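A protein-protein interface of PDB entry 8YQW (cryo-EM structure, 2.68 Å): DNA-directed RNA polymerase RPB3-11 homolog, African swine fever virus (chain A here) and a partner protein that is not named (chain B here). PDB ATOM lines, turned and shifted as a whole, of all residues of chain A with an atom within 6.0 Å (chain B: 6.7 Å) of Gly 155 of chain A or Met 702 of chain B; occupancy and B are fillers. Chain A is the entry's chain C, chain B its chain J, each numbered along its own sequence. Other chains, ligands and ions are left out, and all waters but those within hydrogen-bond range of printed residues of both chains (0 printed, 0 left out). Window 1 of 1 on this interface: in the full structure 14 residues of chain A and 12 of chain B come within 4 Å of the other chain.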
ATOM      1  N   ASP A  82     -10.179 -26.020 -22.704  1.00  0.00           N
ATOM      2  CA  ASP A  82      -8.961 -26.439 -22.033  1.00  0.00           C
ATOM      3  C   ASP A  82      -7.686 -26.020 -22.749  1.00  0.00           C
ATOM      4  O   ASP A  82      -6.653 -25.868 -22.091  1.00  0.00           O
ATOM      5  CB  ASP A  82      -8.952 -27.965 -21.869  1.00  0.00           C
ATOM      6  CG  ASP A  82      -9.894 -28.442 -20.784  1.00  0.00           C
ATOM      7  OD1 ASP A  82     -10.027 -27.740 -19.761  1.00  0.00           O
ATOM      8  OD2 ASP A  82     -10.501 -29.519 -20.958  1.00  0.00           O
ATOM      9  N   THR A  84      -5.606 -23.404 -23.873  1.00  0.00           N
ATOM     10  CA  THR A  84      -5.442 -21.967 -23.705  1.00  0.00           C
ATOM     11  C   THR A  84      -4.378 -21.369 -24.614  1.00  0.00           C
ATOM     12  O   THR A  84      -4.280 -20.140 -24.694  1.00  0.00           O
ATOM     13  CB  THR A  84      -5.092 -21.635 -22.252  1.00  0.00           C
ATOM     14  OG1 THR A  84      -3.932 -22.371 -21.859  1.00  0.00           O
ATOM     15  CG2 THR A  84      -6.244 -21.989 -21.333  1.00  0.00           C
ATOM     16  N   LEU A 116       0.421 -29.662 -20.515  1.00  0.00           N
ATOM     17  CA  LEU A 116       0.349 -28.571 -19.556  1.00  0.00           C
ATOM     18  C   LEU A 116       1.730 -27.947 -19.418  1.00  0.00           C
ATOM     19  O   LEU A 116       2.724 -28.659 -19.253  1.00  0.00           O
ATOM     20  CB  LEU A 116      -0.132 -29.064 -18.183  1.00  0.00           C
ATOM     21  CG  LEU A 116      -1.622 -29.263 -17.886  1.00  0.00           C
ATOM     22  CD1 LEU A 116      -2.369 -27.957 -18.015  1.00  0.00           C
ATOM     23  CD2 LEU A 116      -2.252 -30.331 -18.765  1.00  0.00           C
ATOM     24  N   ASN A 117       1.794 -26.624 -19.475  1.00  0.00           N
ATOM     25  CA  ASN A 117       3.056 -25.897 -19.360  1.00  0.00           C
ATOM     26  C   ASN A 117       3.049 -25.129 -18.042  1.00  0.00           C
ATOM     27  O   ASN A 117       2.473 -24.042 -17.946  1.00  0.00           O
ATOM     28  CB  ASN A 117       3.261 -24.969 -20.553  1.00  0.00           C
ATOM     29  CG  ASN A 117       4.707 -24.573 -20.735  1.00  0.00           C
ATOM     30  OD1 ASN A 117       5.565 -24.938 -19.938  1.00  0.00           O
ATOM     31  ND2 ASN A 117       4.985 -23.821 -21.791  1.00  0.00           N
ATOM     32  N   ASN A 118       3.697 -25.699 -17.031  1.00  0.00           N
ATOM     33  CA  ASN A 118       3.774 -25.106 -15.705  1.00  0.00           C
ATOM     34  C   ASN A 118       5.077 -24.359 -15.468  1.00  0.00           C
ATOM     35  O   ASN A 118       5.402 -24.058 -14.316  1.00  0.00           O
ATOM     36  CB  ASN A 118       3.608 -26.190 -14.639  1.00  0.00           C
ATOM     37  CG  ASN A 118       2.189 -26.696 -14.542  1.00  0.00           C
ATOM     38  OD1 ASN A 118       1.271 -26.116 -15.116  1.00  0.00           O
ATOM     39  ND2 ASN A 118       2.000 -27.791 -13.814  1.00  0.00           N
ATOM     40  N   SER A 119       5.828 -24.058 -16.517  1.00  0.00           N
ATOM     41  CA  SER A 119       7.150 -23.469 -16.391  1.00  0.00           C
ATOM     42  C   SER A 119       7.183 -22.094 -17.048  1.00  0.00           C
ATOM     43  O   SER A 119       6.221 -21.650 -17.681  1.00  0.00           O
ATOM     44  CB  SER A 119       8.205 -24.394 -17.000  1.00  0.00           C
ATOM     45  OG  SER A 119       7.984 -24.576 -18.386  1.00  0.00           O
ATOM     46  N   GLN A 153       3.503 -21.718 -25.081  1.00  0.00           N
ATOM     47  CA  GLN A 153       4.043 -20.596 -24.343  1.00  0.00           C
ATOM     48  C   GLN A 153       3.897 -20.860 -22.847  1.00  0.00           C
ATOM     49  O   GLN A 153       3.107 -21.712 -22.437  1.00  0.00           O
ATOM     50  CB  GLN A 153       3.314 -19.313 -24.734  1.00  0.00           C
ATOM     51  CG  GLN A 153       3.348 -19.010 -26.219  1.00  0.00           C
ATOM     52  CD  GLN A 153       4.740 -18.697 -26.717  1.00  0.00           C
ATOM     53  OE1 GLN A 153       5.445 -17.872 -26.141  1.00  0.00           O
ATOM     54  NE2 GLN A 153       5.146 -19.361 -27.790  1.00  0.00           N
ATOM     55  N   PRO A 154       4.672 -20.168 -22.013  1.00  0.00           N
ATOM     56  CA  PRO A 154       4.580 -20.399 -20.565  1.00  0.00           C
ATOM     57  C   PRO A 154       3.160 -20.212 -20.052  1.00  0.00           C
ATOM     58  O   PRO A 154       2.484 -19.235 -20.381  1.00  0.00           O
ATOM     59  CB  PRO A 154       5.533 -19.353 -19.982  1.00  0.00           C
ATOM     60  CG  PRO A 154       6.506 -19.097 -21.062  1.00  0.00           C
ATOM     61  CD  PRO A 154       5.763 -19.238 -22.350  1.00  0.00           C
ATOM     62  N   GLY A 155       2.711 -21.162 -19.237  1.00  0.00           N
ATOM     63  CA  GLY A 155       1.394 -21.082 -18.642  1.00  0.00           C
ATOM     64  C   GLY A 155       0.241 -21.421 -19.555  1.00  0.00           C
ATOM     65  O   GLY A 155      -0.896 -21.050 -19.253  1.00  0.00           O
ATOM     66  N   LYS A 156       0.491 -22.115 -20.659  1.00  0.00           N
ATOM     67  CA  LYS A 156      -0.543 -22.458 -21.622  1.00  0.00           C
ATOM     68  C   LYS A 156      -0.771 -23.963 -21.645  1.00  0.00           C
ATOM     69  O   LYS A 156       0.001 -24.746 -21.087  1.00  0.00           O
ATOM     70  CB  LYS A 156      -0.174 -21.948 -23.017  1.00  0.00           C
ATOM     71  CG  LYS A 156      -0.053 -20.443 -23.094  1.00  0.00           C
ATOM     72  CD  LYS A 156      -1.303 -19.778 -22.555  1.00  0.00           C
ATOM     73  CE  LYS A 156      -1.177 -18.269 -22.570  1.00  0.00           C
ATOM     74  NZ  LYS A 156      -2.394 -17.619 -22.027  1.00  0.00           N
ATOM     75  N   SER A 157      -1.852 -24.361 -22.312  1.00  0.00           N
ATOM     76  CA  SER A 157      -2.281 -25.750 -22.337  1.00  0.00           C
ATOM     77  C   SER A 157      -2.677 -26.140 -23.752  1.00  0.00           C
ATOM     78  O   SER A 157      -2.973 -25.291 -24.594  1.00  0.00           O
ATOM     79  CB  SER A 157      -3.460 -25.985 -21.388  1.00  0.00           C
ATOM     80  OG  SER A 157      -3.092 -25.724 -20.049  1.00  0.00           O
ATOM     81  N   ALA B 691      -2.420 -13.187 -14.847  1.00  0.00           N
ATOM     82  CA  ALA B 691      -3.048 -14.502 -14.828  1.00  0.00           C
ATOM     83  C   ALA B 691      -2.084 -15.582 -15.299  1.00  0.00           C
ATOM     84  O   ALA B 691      -2.083 -16.695 -14.762  1.00  0.00           O
ATOM     85  CB  ALA B 691      -4.308 -14.494 -15.690  1.00  0.00           C
ATOM     86  N   THR B 692      -1.269 -15.281 -16.311  1.00  0.00           N
ATOM     87  CA  THR B 692      -0.255 -16.234 -16.748  1.00  0.00           C
ATOM     88  C   THR B 692       0.746 -16.515 -15.635  1.00  0.00           C
ATOM     89  O   THR B 692       1.120 -17.671 -15.398  1.00  0.00           O
ATOM     90  CB  THR B 692       0.461 -15.708 -17.990  1.00  0.00           C
ATOM     91  OG1 THR B 692      -0.478 -15.563 -19.061  1.00  0.00           O
ATOM     92  CG2 THR B 692       1.560 -16.662 -18.416  1.00  0.00           C
ATOM     93  N   ARG B 695      -0.902 -18.745 -13.141  1.00  0.00           N
ATOM     94  CA  ARG B 695      -1.017 -20.115 -13.629  1.00  0.00           C
ATOM     95  C   ARG B 695       0.317 -20.847 -13.576  1.00  0.00           C
ATOM     96  O   ARG B 695       0.348 -22.054 -13.310  1.00  0.00           O
ATOM     97  CB  ARG B 695      -1.555 -20.123 -15.060  1.00  0.00           C
ATOM     98  CG  ARG B 695      -3.052 -19.959 -15.163  1.00  0.00           C
ATOM     99  CD  ARG B 695      -3.529 -20.061 -16.597  1.00  0.00           C
ATOM    100  NE  ARG B 695      -4.965 -19.839 -16.701  1.00  0.00           N
ATOM    101  CZ  ARG B 695      -5.524 -18.679 -17.017  1.00  0.00           C
ATOM    102  NH1 ARG B 695      -4.792 -17.611 -17.282  1.00  0.00           N
ATOM    103  NH2 ARG B 695      -6.849 -18.589 -17.071  1.00  0.00           N
ATOM    104  N   ILE B 696       1.419 -20.140 -13.837  1.00  0.00           N
ATOM    105  CA  ILE B 696       2.728 -20.787 -13.906  1.00  0.00           C
ATOM    106  C   ILE B 696       3.071 -21.461 -12.582  1.00  0.00           C
ATOM    107  O   ILE B 696       3.627 -22.566 -12.559  1.00  0.00           O
ATOM    108  CB  ILE B 696       3.803 -19.764 -14.323  1.00  0.00           C
ATOM    109  CG1 ILE B 696       3.832 -19.622 -15.845  1.00  0.00           C
ATOM    110  CG2 ILE B 696       5.170 -20.161 -13.795  1.00  0.00           C
ATOM    111  CD1 ILE B 696       4.737 -18.518 -16.336  1.00  0.00           C
ATOM    112  N   GLY B 698       0.701 -22.231 -10.255  1.00  0.00           N
ATOM    113  CA  GLY B 698      -0.419 -23.016  -9.775  1.00  0.00           C
ATOM    114  C   GLY B 698      -1.396 -22.306  -8.866  1.00  0.00           C
ATOM    115  O   GLY B 698      -2.237 -22.975  -8.256  1.00  0.00           O
ATOM    116  N   ILE B 700      -3.836 -20.379  -9.735  1.00  0.00           N
ATOM    117  CA  ILE B 700      -5.156 -20.463 -10.357  1.00  0.00           C
ATOM    118  C   ILE B 700      -5.150 -21.631 -11.334  1.00  0.00           C
ATOM    119  O   ILE B 700      -4.084 -22.057 -11.807  1.00  0.00           O
ATOM    120  CB  ILE B 700      -5.540 -19.142 -11.066  1.00  0.00           C
ATOM    121  CG1 ILE B 700      -4.515 -18.794 -12.146  1.00  0.00           C
ATOM    122  CG2 ILE B 700      -5.667 -18.013 -10.063  1.00  0.00           C
ATOM    123  CD1 ILE B 700      -4.916 -17.626 -13.012  1.00  0.00           C
ATOM    124  N   PRO B 701      -6.325 -22.185 -11.643  1.00  0.00           N
ATOM    125  CA  PRO B 701      -6.380 -23.309 -12.585  1.00  0.00           C
ATOM    126  C   PRO B 701      -5.836 -22.933 -13.955  1.00  0.00           C
ATOM    127  O   PRO B 701      -5.977 -21.800 -14.418  1.00  0.00           O
ATOM    128  CB  PRO B 701      -7.875 -23.645 -12.650  1.00  0.00           C
ATOM    129  CG  PRO B 701      -8.434 -23.127 -11.379  1.00  0.00           C
ATOM    130  CD  PRO B 701      -7.641 -21.904 -11.045  1.00  0.00           C
ATOM    131  N   MET B 702      -5.210 -23.915 -14.609  1.00  0.00           N
ATOM    132  CA  MET B 702      -4.564 -23.695 -15.897  1.00  0.00           C
ATOM    133  C   MET B 702      -5.550 -23.430 -17.026  1.00  0.00           C
ATOM    134  O   MET B 702      -5.124 -23.018 -18.110  1.00  0.00           O
ATOM    135  CB  MET B 702      -3.688 -24.896 -16.255  1.00  0.00           C
ATOM    136  CG  MET B 702      -2.413 -24.997 -15.436  1.00  0.00           C
ATOM    137  SD  MET B 702      -1.111 -23.908 -16.041  1.00  0.00           S
ATOM    138  CE  MET B 702      -0.691 -24.705 -17.584  1.00  0.00           C
ATOM    139  N   HIS B 703      -6.840 -23.657 -16.809  1.00  0.00           N
ATOM    140  CA  HIS B 703      -7.863 -23.376 -17.803  1.00  0.00           C
ATOM    141  C   HIS B 703      -8.602 -22.090 -17.454  1.00  0.00           C
ATOM    142  O   HIS B 703      -8.575 -21.618 -16.316  1.00  0.00           O
ATOM    143  CB  HIS B 703      -8.852 -24.540 -17.907  1.00  0.00           C
ATOM    144  CG  HIS B 703      -9.451 -24.946 -16.596  1.00  0.00           C
ATOM    145  ND1 HIS B 703     -10.212 -24.092 -15.827  1.00  0.00           N
ATOM    146  CD2 HIS B 703      -9.395 -26.114 -15.915  1.00  0.00           C
ATOM    147  CE1 HIS B 703     -10.602 -24.718 -14.732  1.00  0.00           C
ATOM    148  NE2 HIS B 703     -10.120 -25.947 -14.761  1.00  0.00           N
ATOM    149  N   LYS B 704      -9.270 -21.528 -18.456  1.00  0.00           N
ATOM    150  CA  LYS B 704     -10.072 -20.340 -18.241  1.00  0.00           C
ATOM    151  C   LYS B 704     -11.270 -20.673 -17.355  1.00  0.00           C
ATOM    152  O   LYS B 704     -11.720 -21.820 -17.308  1.00  0.00           O
ATOM    153  CB  LYS B 704     -10.548 -19.772 -19.575  1.00  0.00           C
ATOM    154  CG  LYS B 704      -9.431 -19.346 -20.506  1.00  0.00           C
ATOM    155  CD  LYS B 704      -9.992 -18.696 -21.762  1.00  0.00           C
ATOM    156  CE  LYS B 704     -10.663 -19.718 -22.670  1.00  0.00           C
ATOM    157  NZ  LYS B 704      -9.683 -20.668 -23.270  1.00  0.00           N
ATOM    158  N   TYR B 778      12.176 -14.240 -17.506  1.00  0.00           N
ATOM    159  CA  TYR B 778      10.722 -14.097 -17.469  1.00  0.00           C
ATOM    160  C   TYR B 778      10.258 -13.471 -16.157  1.00  0.00           C
ATOM    161  O   TYR B 778       9.472 -12.511 -16.148  1.00  0.00           O
ATOM    162  CB  TYR B 778      10.067 -15.464 -17.677  1.00  0.00           C
ATOM    163  CG  TYR B 778       8.590 -15.415 -17.989  1.00  0.00           C
ATOM    164  CD1 TYR B 778       7.645 -15.400 -16.972  1.00  0.00           C
ATOM    165  CD2 TYR B 778       8.138 -15.391 -19.299  1.00  0.00           C
ATOM    166  CE1 TYR B 778       6.296 -15.356 -17.253  1.00  0.00           C
ATOM    167  CE2 TYR B 778       6.792 -15.349 -19.588  1.00  0.00           C
ATOM    168  CZ  TYR B 778       5.876 -15.332 -18.563  1.00  0.00           C
ATOM    169  OH  TYR B 778       4.533 -15.290 -18.849  1.00  0.00           O
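The side-chain amide oxygen (OD1) of Asn 118 of chain A lies close to the side-chain sulfur (SD) of Met 702 of chain B.
The backbone carbonyl oxygen of Ile 696 of chain B lies close to the backbone carbonyl oxygen of Asn 118 of chain A (2.9 Å).
The backbone NH of Ser 157 of chain A is in hydrogen-bond range of the side-chain hydroxyl of Thr 84 of chain A.
The side-chain hydroxyl (OG) of Ser 119 of chain A lies within hydrogen-bond range of the side-chain amide oxygen (OD1) of Asn 117 of chain A (2.9 Å).
The side-chain amide nitrogen (ND2) of Asn 117 of chain A sits at hydrogen-bond distance from the backbone carbonyl oxygen (O) of Gln 153 of chain A (2.9 Å).
O of Asn 117 of chain A sits at hydrogen-bond distance from N of Gly 155 of chain A (3.2 Å).
The backbone NH (N) of Asn 117 of chain A sits at hydrogen-bond distance from the backbone carbonyl oxygen (O) of Lys 156 of chain A (3.1 Å).
The guanidinium group (NE) of Arg 695 of chain B is in hydrogen-bond range of the backbone carbonyl oxygen (O) of Pro 701 of chain B.
Of the 11 printed residues of chain B, 5 touch a printed residue of chain A.
Printed residues of chain B that touch a printed residue of chain A: Thr 692, Arg 695, Ile 696, Met 702 and His 703.
Hydrophobic or aromatic side chains of chain B within 4 Å of the printed part of chain A: Ile 696, Met 702 and His 703.
Printed residues of chain A that touch a printed residue of chain B: Asp 82, Thr 84, Leu 116, Asn 117, Asn 118, Ser 119, Pro 154, Gly 155, Lys 156 and Ser 157.
Hydrophobic or aromatic side chains of chain A that line the printed part of chain B: Leu 116 and Pro 154.
Among the printed residues, 14 pairs touch across the chains.
Among the printed residues, no Asp or Glu carboxylate lies within 4 Å of a Lys or Arg side-chain nitrogen of the other chain.
Among the printed residues, merely in contact across the chains: Asp 82 of chain A with His 703 of chain B, Thr 84 of chain A with Met 702 of chain B, Leu 116 of chain A with Met 702 of chain B, Asn 117 of chain A with Met 702 of chain B, Ser 119 of chain A with Ile 696 of chain B, Pro 154 of chain A with Thr 692 of chain B, Pro 154 of chain A with Ile 696 of chain B, Gly 155 of chain A with Arg 695 of chain B, Gly 155 of chain A with Ile 696 of chain B, Gly 155 of chain A with Met 702 of chain B, Lys 156 of chain A with Met 702 of chain B and Ser 157 of chain A with Met 702 of chain B.
Of the printed residues of chain B, Asp 82 of chain A touches His 703.
Of the printed residues of chain B, Pro 154 of chain A touches Thr 692 and Ile 696.
Gly 155 of chain A touches just these residues of chain B: Arg 695, Ile 696 and Met 702.
Ile 700 of chain B touches none of the printed residues of chain A.
Pro 701 of chain B touches none of the printed residues of chain A.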
